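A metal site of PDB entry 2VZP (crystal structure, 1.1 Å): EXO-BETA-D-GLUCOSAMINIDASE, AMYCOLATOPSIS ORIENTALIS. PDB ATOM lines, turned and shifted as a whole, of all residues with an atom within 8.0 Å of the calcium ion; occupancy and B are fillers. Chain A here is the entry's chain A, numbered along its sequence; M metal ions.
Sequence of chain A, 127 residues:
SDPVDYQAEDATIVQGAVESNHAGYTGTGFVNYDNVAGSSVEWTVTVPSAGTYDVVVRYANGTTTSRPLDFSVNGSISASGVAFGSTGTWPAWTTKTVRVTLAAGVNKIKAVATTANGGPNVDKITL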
ATOM      1  N   TYR A   6      -1.811   6.900  -1.201  1.00  0.00           N
ATOM      2  CA  TYR A   6      -3.157   6.491  -1.581  1.00  0.00           C
ATOM      3  C   TYR A   6      -4.075   7.021  -0.489  1.00  0.00           C
ATOM      4  O   TYR A   6      -4.145   6.479   0.628  1.00  0.00           O
ATOM      5  CB  TYR A   6      -3.285   5.003  -1.759  1.00  0.00           C
ATOM      6  CG  TYR A   6      -2.379   4.443  -2.835  1.00  0.00           C
ATOM      7  CD1 TYR A   6      -1.126   3.959  -2.535  1.00  0.00           C
ATOM      8  CD2 TYR A   6      -2.804   4.395  -4.142  1.00  0.00           C
ATOM      9  CE1 TYR A   6      -0.265   3.393  -3.533  1.00  0.00           C
ATOM     10  CE2 TYR A   6      -1.974   3.856  -5.144  1.00  0.00           C
ATOM     11  CZ  TYR A   6      -0.724   3.373  -4.808  1.00  0.00           C
ATOM     12  OH  TYR A   6       0.025   2.789  -5.804  1.00  0.00           O
ATOM     13  N   GLN A   7      -4.760   8.133  -0.764  1.00  0.00           N
ATOM     14  CA  GLN A   7      -5.545   8.811   0.270  1.00  0.00           C
ATOM     15  C   GLN A   7      -6.777   7.998   0.625  1.00  0.00           C
ATOM     16  O   GLN A   7      -7.495   7.500  -0.249  1.00  0.00           O
ATOM     17  CB  GLN A   7      -5.938  10.211  -0.243  1.00  0.00           C
ATOM     18  CG  GLN A   7      -4.761  11.125  -0.459  1.00  0.00           C
ATOM     19  CD  GLN A   7      -4.036  11.481   0.821  1.00  0.00           C
ATOM     20  OE1 GLN A   7      -4.604  11.319   1.933  1.00  0.00           O
ATOM     21  NE2 GLN A   7      -2.774  11.961   0.746  1.00  0.00           N
ATOM     22  N   ALA A   8      -7.046   7.879   1.921  1.00  0.00           N
ATOM     23  CA  ALA A   8      -8.212   7.093   2.389  1.00  0.00           C
ATOM     24  C   ALA A   8      -9.518   7.628   1.853  1.00  0.00           C
ATOM     25  O   ALA A   8     -10.443   6.905   1.510  1.00  0.00           O
ATOM     26  CB  ALA A   8      -8.214   7.078   3.895  1.00  0.00           C
ATOM     27  N   GLU A   9      -9.619   8.968   1.801  1.00  0.00           N
ATOM     28  CA  GLU A   9     -10.862   9.632   1.396  1.00  0.00           C
ATOM     29  C   GLU A   9     -11.171   9.401  -0.064  1.00  0.00           C
ATOM     30  O   GLU A   9     -12.319   9.631  -0.487  1.00  0.00           O
ATOM     31  CB  GLU A   9     -10.786  11.146   1.714  1.00  0.00           C
ATOM     32  CG  GLU A   9      -9.606  11.899   1.075  1.00  0.00           C
ATOM     33  CD  GLU A   9      -8.320  11.928   1.861  1.00  0.00           C
ATOM     34  OE1 GLU A   9      -8.064  11.012   2.730  1.00  0.00           O
ATOM     35  OE2 GLU A   9      -7.488  12.825   1.666  1.00  0.00           O
ATOM     36  N   ASP A  10     -10.208   8.888  -0.858  1.00  0.00           N
ATOM     37  CA  ASP A  10     -10.412   8.561  -2.297  1.00  0.00           C
ATOM     38  C   ASP A  10     -10.590   7.085  -2.560  1.00  0.00           C
ATOM     39  O   ASP A  10     -10.702   6.677  -3.733  1.00  0.00           O
ATOM     40  CB  ASP A  10      -9.250   9.152  -3.095  1.00  0.00           C
ATOM     41  CG  ASP A  10      -9.199  10.659  -2.965  1.00  0.00           C
ATOM     42  OD1 ASP A  10     -10.223  11.290  -3.035  1.00  0.00           O
ATOM     43  OD2 ASP A  10      -8.162  11.216  -2.664  1.00  0.00           O
ATOM     44  N   VAL A  18     -15.956  10.636   5.200  1.00  0.00           N
ATOM     45  CA  VAL A  18     -14.865  11.512   4.897  1.00  0.00           C
ATOM     46  C   VAL A  18     -15.038  12.778   5.713  1.00  0.00           C
ATOM     47  O   VAL A  18     -16.085  13.447   5.635  1.00  0.00           O
ATOM     48  CB  VAL A  18     -14.834  11.877   3.403  1.00  0.00           C
ATOM     49  CG1 VAL A  18     -13.773  12.926   3.138  1.00  0.00           C
ATOM     50  CG2 VAL A  18     -14.546  10.613   2.596  1.00  0.00           C
ATOM     51  N   GLU A  19     -14.037  13.148   6.498  1.00  0.00           N
ATOM     52  CA  GLU A  19     -14.045  14.289   7.359  1.00  0.00           C
ATOM     53  C   GLU A  19     -12.740  15.055   7.256  1.00  0.00           C
ATOM     54  O   GLU A  19     -11.753  14.614   6.669  1.00  0.00           O
ATOM     55  CB  GLU A  19     -14.391  13.896   8.814  1.00  0.00           C
ATOM     56  CG  GLU A  19     -15.802  13.300   8.860  1.00  0.00           C
ATOM     57  CD  GLU A  19     -16.314  12.780  10.139  1.00  0.00           C
ATOM     58  OE1 GLU A  19     -15.544  12.637  11.095  1.00  0.00           O
ATOM     59  OE2 GLU A  19     -17.544  12.484  10.226  1.00  0.00           O
ATOM     60  N   GLY A  24      -4.012  18.391  10.161  1.00  0.00           N
ATOM     61  CA  GLY A  24      -2.808  17.647   9.890  1.00  0.00           C
ATOM     62  C   GLY A  24      -2.919  16.473   8.928  1.00  0.00           C
ATOM     63  O   GLY A  24      -1.922  15.774   8.676  1.00  0.00           O
ATOM     64  N   TYR A  25      -4.108  16.215   8.433  1.00  0.00           N
ATOM     65  CA  TYR A  25      -4.285  15.227   7.366  1.00  0.00           C
ATOM     66  C   TYR A  25      -3.561  15.681   6.107  1.00  0.00           C
ATOM     67  O   TYR A  25      -3.207  16.857   5.953  1.00  0.00           O
ATOM     68  CB  TYR A  25      -5.776  14.959   7.145  1.00  0.00           C
ATOM     69  CG  TYR A  25      -6.552  16.182   6.745  1.00  0.00           C
ATOM     70  CD1 TYR A  25      -6.528  16.678   5.447  1.00  0.00           C
ATOM     71  CD2 TYR A  25      -7.324  16.868   7.716  1.00  0.00           C
ATOM     72  CE1 TYR A  25      -7.214  17.839   5.103  1.00  0.00           C
ATOM     73  CE2 TYR A  25      -8.020  18.021   7.399  1.00  0.00           C
ATOM     74  CZ  TYR A  25      -7.951  18.507   6.121  1.00  0.00           C
ATOM     75  OH  TYR A  25      -8.661  19.665   5.833  1.00  0.00           O
ATOM     76  N   THR A  26      -3.374  14.744   5.176  1.00  0.00           N
ATOM     77  CA  THR A  26      -2.874  15.035   3.835  1.00  0.00           C
ATOM     78  C   THR A  26      -4.011  14.734   2.853  1.00  0.00           C
ATOM     79  O   THR A  26      -5.035  14.119   3.188  1.00  0.00           O
ATOM     80  CB  THR A  26      -1.620  14.247   3.522  1.00  0.00           C
ATOM     81  OG1 THR A  26      -1.886  12.826   3.468  1.00  0.00           O
ATOM     82  CG2 THR A  26      -0.500  14.531   4.523  1.00  0.00           C
ATOM     83  N   GLY A  27      -3.863  15.223   1.634  1.00  0.00           N
ATOM     84  CA  GLY A  27      -4.980  15.192   0.714  1.00  0.00           C
ATOM     85  C   GLY A  27      -6.068  16.109   1.189  1.00  0.00           C
ATOM     86  O   GLY A  27      -5.805  17.088   1.868  1.00  0.00           O
ATOM     87  N   THR A  28      -7.305  15.840   0.835  1.00  0.00           N
ATOM     88  CA  THR A  28      -8.410  16.714   1.174  1.00  0.00           C
ATOM     89  C   THR A  28      -9.090  16.362   2.501  1.00  0.00           C
ATOM     90  O   THR A  28      -9.950  17.142   2.963  1.00  0.00           O
ATOM     91  CB  THR A  28      -9.481  16.693   0.026  1.00  0.00           C
ATOM     92  OG1 THR A  28      -9.916  15.372  -0.206  1.00  0.00           O
ATOM     93  CG2 THR A  28      -8.906  17.369  -1.239  1.00  0.00           C
ATOM     94  N   GLY A  29      -8.742  15.257   3.152  1.00  0.00           N
ATOM     95  CA  GLY A  29      -9.352  14.903   4.416  1.00  0.00           C
ATOM     96  C   GLY A  29      -8.835  13.582   4.902  1.00  0.00           C
ATOM     97  O   GLY A  29      -7.670  13.222   4.698  1.00  0.00           O
ATOM     98  N   PHE A  30      -9.708  12.853   5.593  1.00  0.00           N
ATOM     99  CA  PHE A  30      -9.367  11.532   6.163  1.00  0.00           C
ATOM    100  C   PHE A  30     -10.685  10.771   6.295  1.00  0.00           C
ATOM    101  O   PHE A  30     -11.765  11.336   6.141  1.00  0.00           O
ATOM    102  CB  PHE A  30      -8.618  11.651   7.495  1.00  0.00           C
ATOM    103  CG  PHE A  30      -9.369  12.447   8.535  1.00  0.00           C
ATOM    104  CD1 PHE A  30     -10.297  11.878   9.376  1.00  0.00           C
ATOM    105  CD2 PHE A  30      -9.156  13.823   8.652  1.00  0.00           C
ATOM    106  CE1 PHE A  30     -10.986  12.605  10.319  1.00  0.00           C
ATOM    107  CE2 PHE A  30      -9.840  14.562   9.626  1.00  0.00           C
ATOM    108  CZ  PHE A  30     -10.755  13.951  10.474  1.00  0.00           C
ATOM    109  N   VAL A  31     -10.578   9.476   6.629  1.00  0.00           N
ATOM    110  CA  VAL A  31     -11.743   8.673   6.886  1.00  0.00           C
ATOM    111  C   VAL A  31     -11.882   8.439   8.372  1.00  0.00           C
ATOM    112  O   VAL A  31     -10.950   7.974   9.059  1.00  0.00           O
ATOM    113  CB  VAL A  31     -11.699   7.337   6.127  1.00  0.00           C
ATOM    114  CG1 VAL A  31     -12.865   6.437   6.547  1.00  0.00           C
ATOM    115  CG2 VAL A  31     -11.718   7.632   4.628  1.00  0.00           C
ATOM    116  N   TRP A  43      -8.278   0.331  -0.570  1.00  0.00           N
ATOM    117  CA  TRP A  43      -7.481   1.092  -1.515  1.00  0.00           C
ATOM    118  C   TRP A  43      -7.138   0.260  -2.740  1.00  0.00           C
ATOM    119  O   TRP A  43      -6.879  -0.937  -2.624  1.00  0.00           O
ATOM    120  CB  TRP A  43      -6.150   1.486  -0.858  1.00  0.00           C
ATOM    121  CG  TRP A  43      -6.241   2.467   0.283  1.00  0.00           C
ATOM    122  CD1 TRP A  43      -6.087   3.785   0.173  1.00  0.00           C
ATOM    123  CD2 TRP A  43      -6.448   2.181   1.659  1.00  0.00           C
ATOM    124  NE1 TRP A  43      -6.189   4.373   1.410  1.00  0.00           N
ATOM    125  CE2 TRP A  43      -6.377   3.410   2.350  1.00  0.00           C
ATOM    126  CE3 TRP A  43      -6.666   1.036   2.401  1.00  0.00           C
ATOM    127  CZ2 TRP A  43      -6.549   3.515   3.738  1.00  0.00           C
ATOM    128  CZ3 TRP A  43      -6.808   1.114   3.792  1.00  0.00           C
ATOM    129  CH2 TRP A  43      -6.747   2.354   4.435  1.00  0.00           C
ATOM    130  N   ARG A  58      -1.121   5.876   7.907  1.00  0.00           N
ATOM    131  CA  ARG A  58      -1.074   7.126   8.688  1.00  0.00           C
ATOM    132  C   ARG A  58      -2.447   7.313   9.339  1.00  0.00           C
ATOM    133  O   ARG A  58      -3.460   7.366   8.629  1.00  0.00           O
ATOM    134  CB  ARG A  58      -0.689   8.309   7.796  1.00  0.00           C
ATOM    135  CG  ARG A  58      -0.414   9.567   8.604  1.00  0.00           C
ATOM    136  CD  ARG A  58       0.218  10.649   7.706  1.00  0.00           C
ATOM    137  NE  ARG A  58       0.672  11.827   8.459  1.00  0.00           N
ATOM    138  CZ  ARG A  58      -0.016  12.953   8.582  1.00  0.00           C
ATOM    139  NH1 ARG A  58      -1.195  13.086   8.041  1.00  0.00           N
ATOM    140  NH2 ARG A  58       0.497  13.973   9.272  1.00  0.00           N
ATOM    141  N   TRP A  93      -1.269  12.626  14.049  1.00  0.00           N
ATOM    142  CA  TRP A  93      -1.177  11.544  13.062  1.00  0.00           C
ATOM    143  C   TRP A  93       0.149  10.808  13.255  1.00  0.00           C
ATOM    144  O   TRP A  93       1.232  11.431  13.352  1.00  0.00           O
ATOM    145  CB  TRP A  93      -1.244  12.121  11.633  1.00  0.00           C
ATOM    146  CG  TRP A  93      -2.545  12.832  11.365  1.00  0.00           C
ATOM    147  CD1 TRP A  93      -2.788  14.146  11.485  1.00  0.00           C
ATOM    148  CD2 TRP A  93      -3.790  12.210  11.021  1.00  0.00           C
ATOM    149  NE1 TRP A  93      -4.102  14.426  11.227  1.00  0.00           N
ATOM    150  CE2 TRP A  93      -4.740  13.251  10.924  1.00  0.00           C
ATOM    151  CE3 TRP A  93      -4.198  10.880  10.766  1.00  0.00           C
ATOM    152  CZ2 TRP A  93      -6.071  13.007  10.588  1.00  0.00           C
ATOM    153  CZ3 TRP A  93      -5.509  10.631  10.451  1.00  0.00           C
ATOM    154  CH2 TRP A  93      -6.418  11.680  10.349  1.00  0.00           C
ATOM    155  N   VAL A 122      -8.150   7.284   9.576  1.00  0.00           N
ATOM    156  CA  VAL A 122      -7.072   6.934   8.648  1.00  0.00           C
ATOM    157  C   VAL A 122      -6.940   7.997   7.588  1.00  0.00           C
ATOM    158  O   VAL A 122      -7.911   8.358   6.897  1.00  0.00           O
ATOM    159  CB  VAL A 122      -7.257   5.524   8.030  1.00  0.00           C
ATOM    160  CG1 VAL A 122      -6.109   5.262   7.040  1.00  0.00           C
ATOM    161  CG2 VAL A 122      -7.293   4.453   9.112  1.00  0.00           C
ATOM    162  N   ASP A 123      -5.746   8.555   7.489  1.00  0.00           N
ATOM    163  CA  ASP A 123      -5.439   9.613   6.510  1.00  0.00           C
ATOM    164  C   ASP A 123      -5.179   9.031   5.119  1.00  0.00           C
ATOM    165  O   ASP A 123      -5.668   9.568   4.121  1.00  0.00           O
ATOM    166  CB  ASP A 123      -4.228  10.367   6.992  1.00  0.00           C
ATOM    167  CG  ASP A 123      -3.786  11.462   6.028  1.00  0.00           C
ATOM    168  OD1 ASP A 123      -4.677  12.102   5.423  1.00  0.00           O
ATOM    169  OD2 ASP A 123      -2.559  11.707   5.925  1.00  0.00           O
ATOM    170  N   LYS A 124      -4.364   7.990   5.027  1.00  0.00           N
ATOM    171  CA  LYS A 124      -3.832   7.444   3.804  1.00  0.00           C
ATOM    172  C   LYS A 124      -3.037   6.179   4.139  1.00  0.00           C
ATOM    173  O   LYS A 124      -2.704   5.936   5.315  1.00  0.00           O
ATOM    174  CB  LYS A 124      -2.897   8.433   3.095  1.00  0.00           C
ATOM    175  CG  LYS A 124      -1.670   8.824   3.872  1.00  0.00           C
ATOM    176  CD  LYS A 124      -0.717   9.697   3.035  1.00  0.00           C
ATOM    177  CE  LYS A 124       0.362  10.315   3.915  1.00  0.00           C
ATOM    178  NZ  LYS A 124       1.302  11.178   3.155  1.00  0.00           N
ATOM    179  N   ILE A 125      -2.686   5.441   3.088  1.00  0.00           N
ATOM    180  CA  ILE A 125      -1.589   4.477   3.129  1.00  0.00           C
ATOM    181  C   ILE A 125      -0.572   4.922   2.088  1.00  0.00           C
ATOM    182  O   ILE A 125      -0.918   5.596   1.118  1.00  0.00           O
ATOM    183  CB  ILE A 125      -2.043   3.029   2.888  1.00  0.00           C
ATOM    184  CG1 ILE A 125      -2.605   2.814   1.477  1.00  0.00           C
ATOM    185  CG2 ILE A 125      -2.987   2.568   3.999  1.00  0.00           C
ATOM    186  CD1 ILE A 125      -2.927   1.332   1.176  1.00  0.00           C
HETATM  187 CA    CA M   1      -6.019  12.042   3.539  1.00  0.00          CA
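The backbone NH (N) of Ala 8 lies close to the backbone carbonyl oxygen (O) of Asp 123 (3.1 Å). The side-chain carboxylate (OE2) of Glu 9 lies close to the backbone NH (N) of Thr 28, 3.1 Å away. NH1 of Arg 58 is in salt-bridge range of OD2 of Asp 123, at 2.9 Å.
Five residues have an atom within 4 Å of the calcium ion: Gln 7, Glu 9, Thr 26, Gly 29 and Asp 123.
The calcium ion is bound by OE1 of Gln 7 (2.3 Å), OD1 of Asp 123 (2.3 Å), O of Thr 26 (2.3 Å), O of Gly 29 (2.3 Å), OE1 of Glu 9 (2.4 Å), OE2 of Glu 9 (2.5 Å) and O of Asp 123 (2.6 Å).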
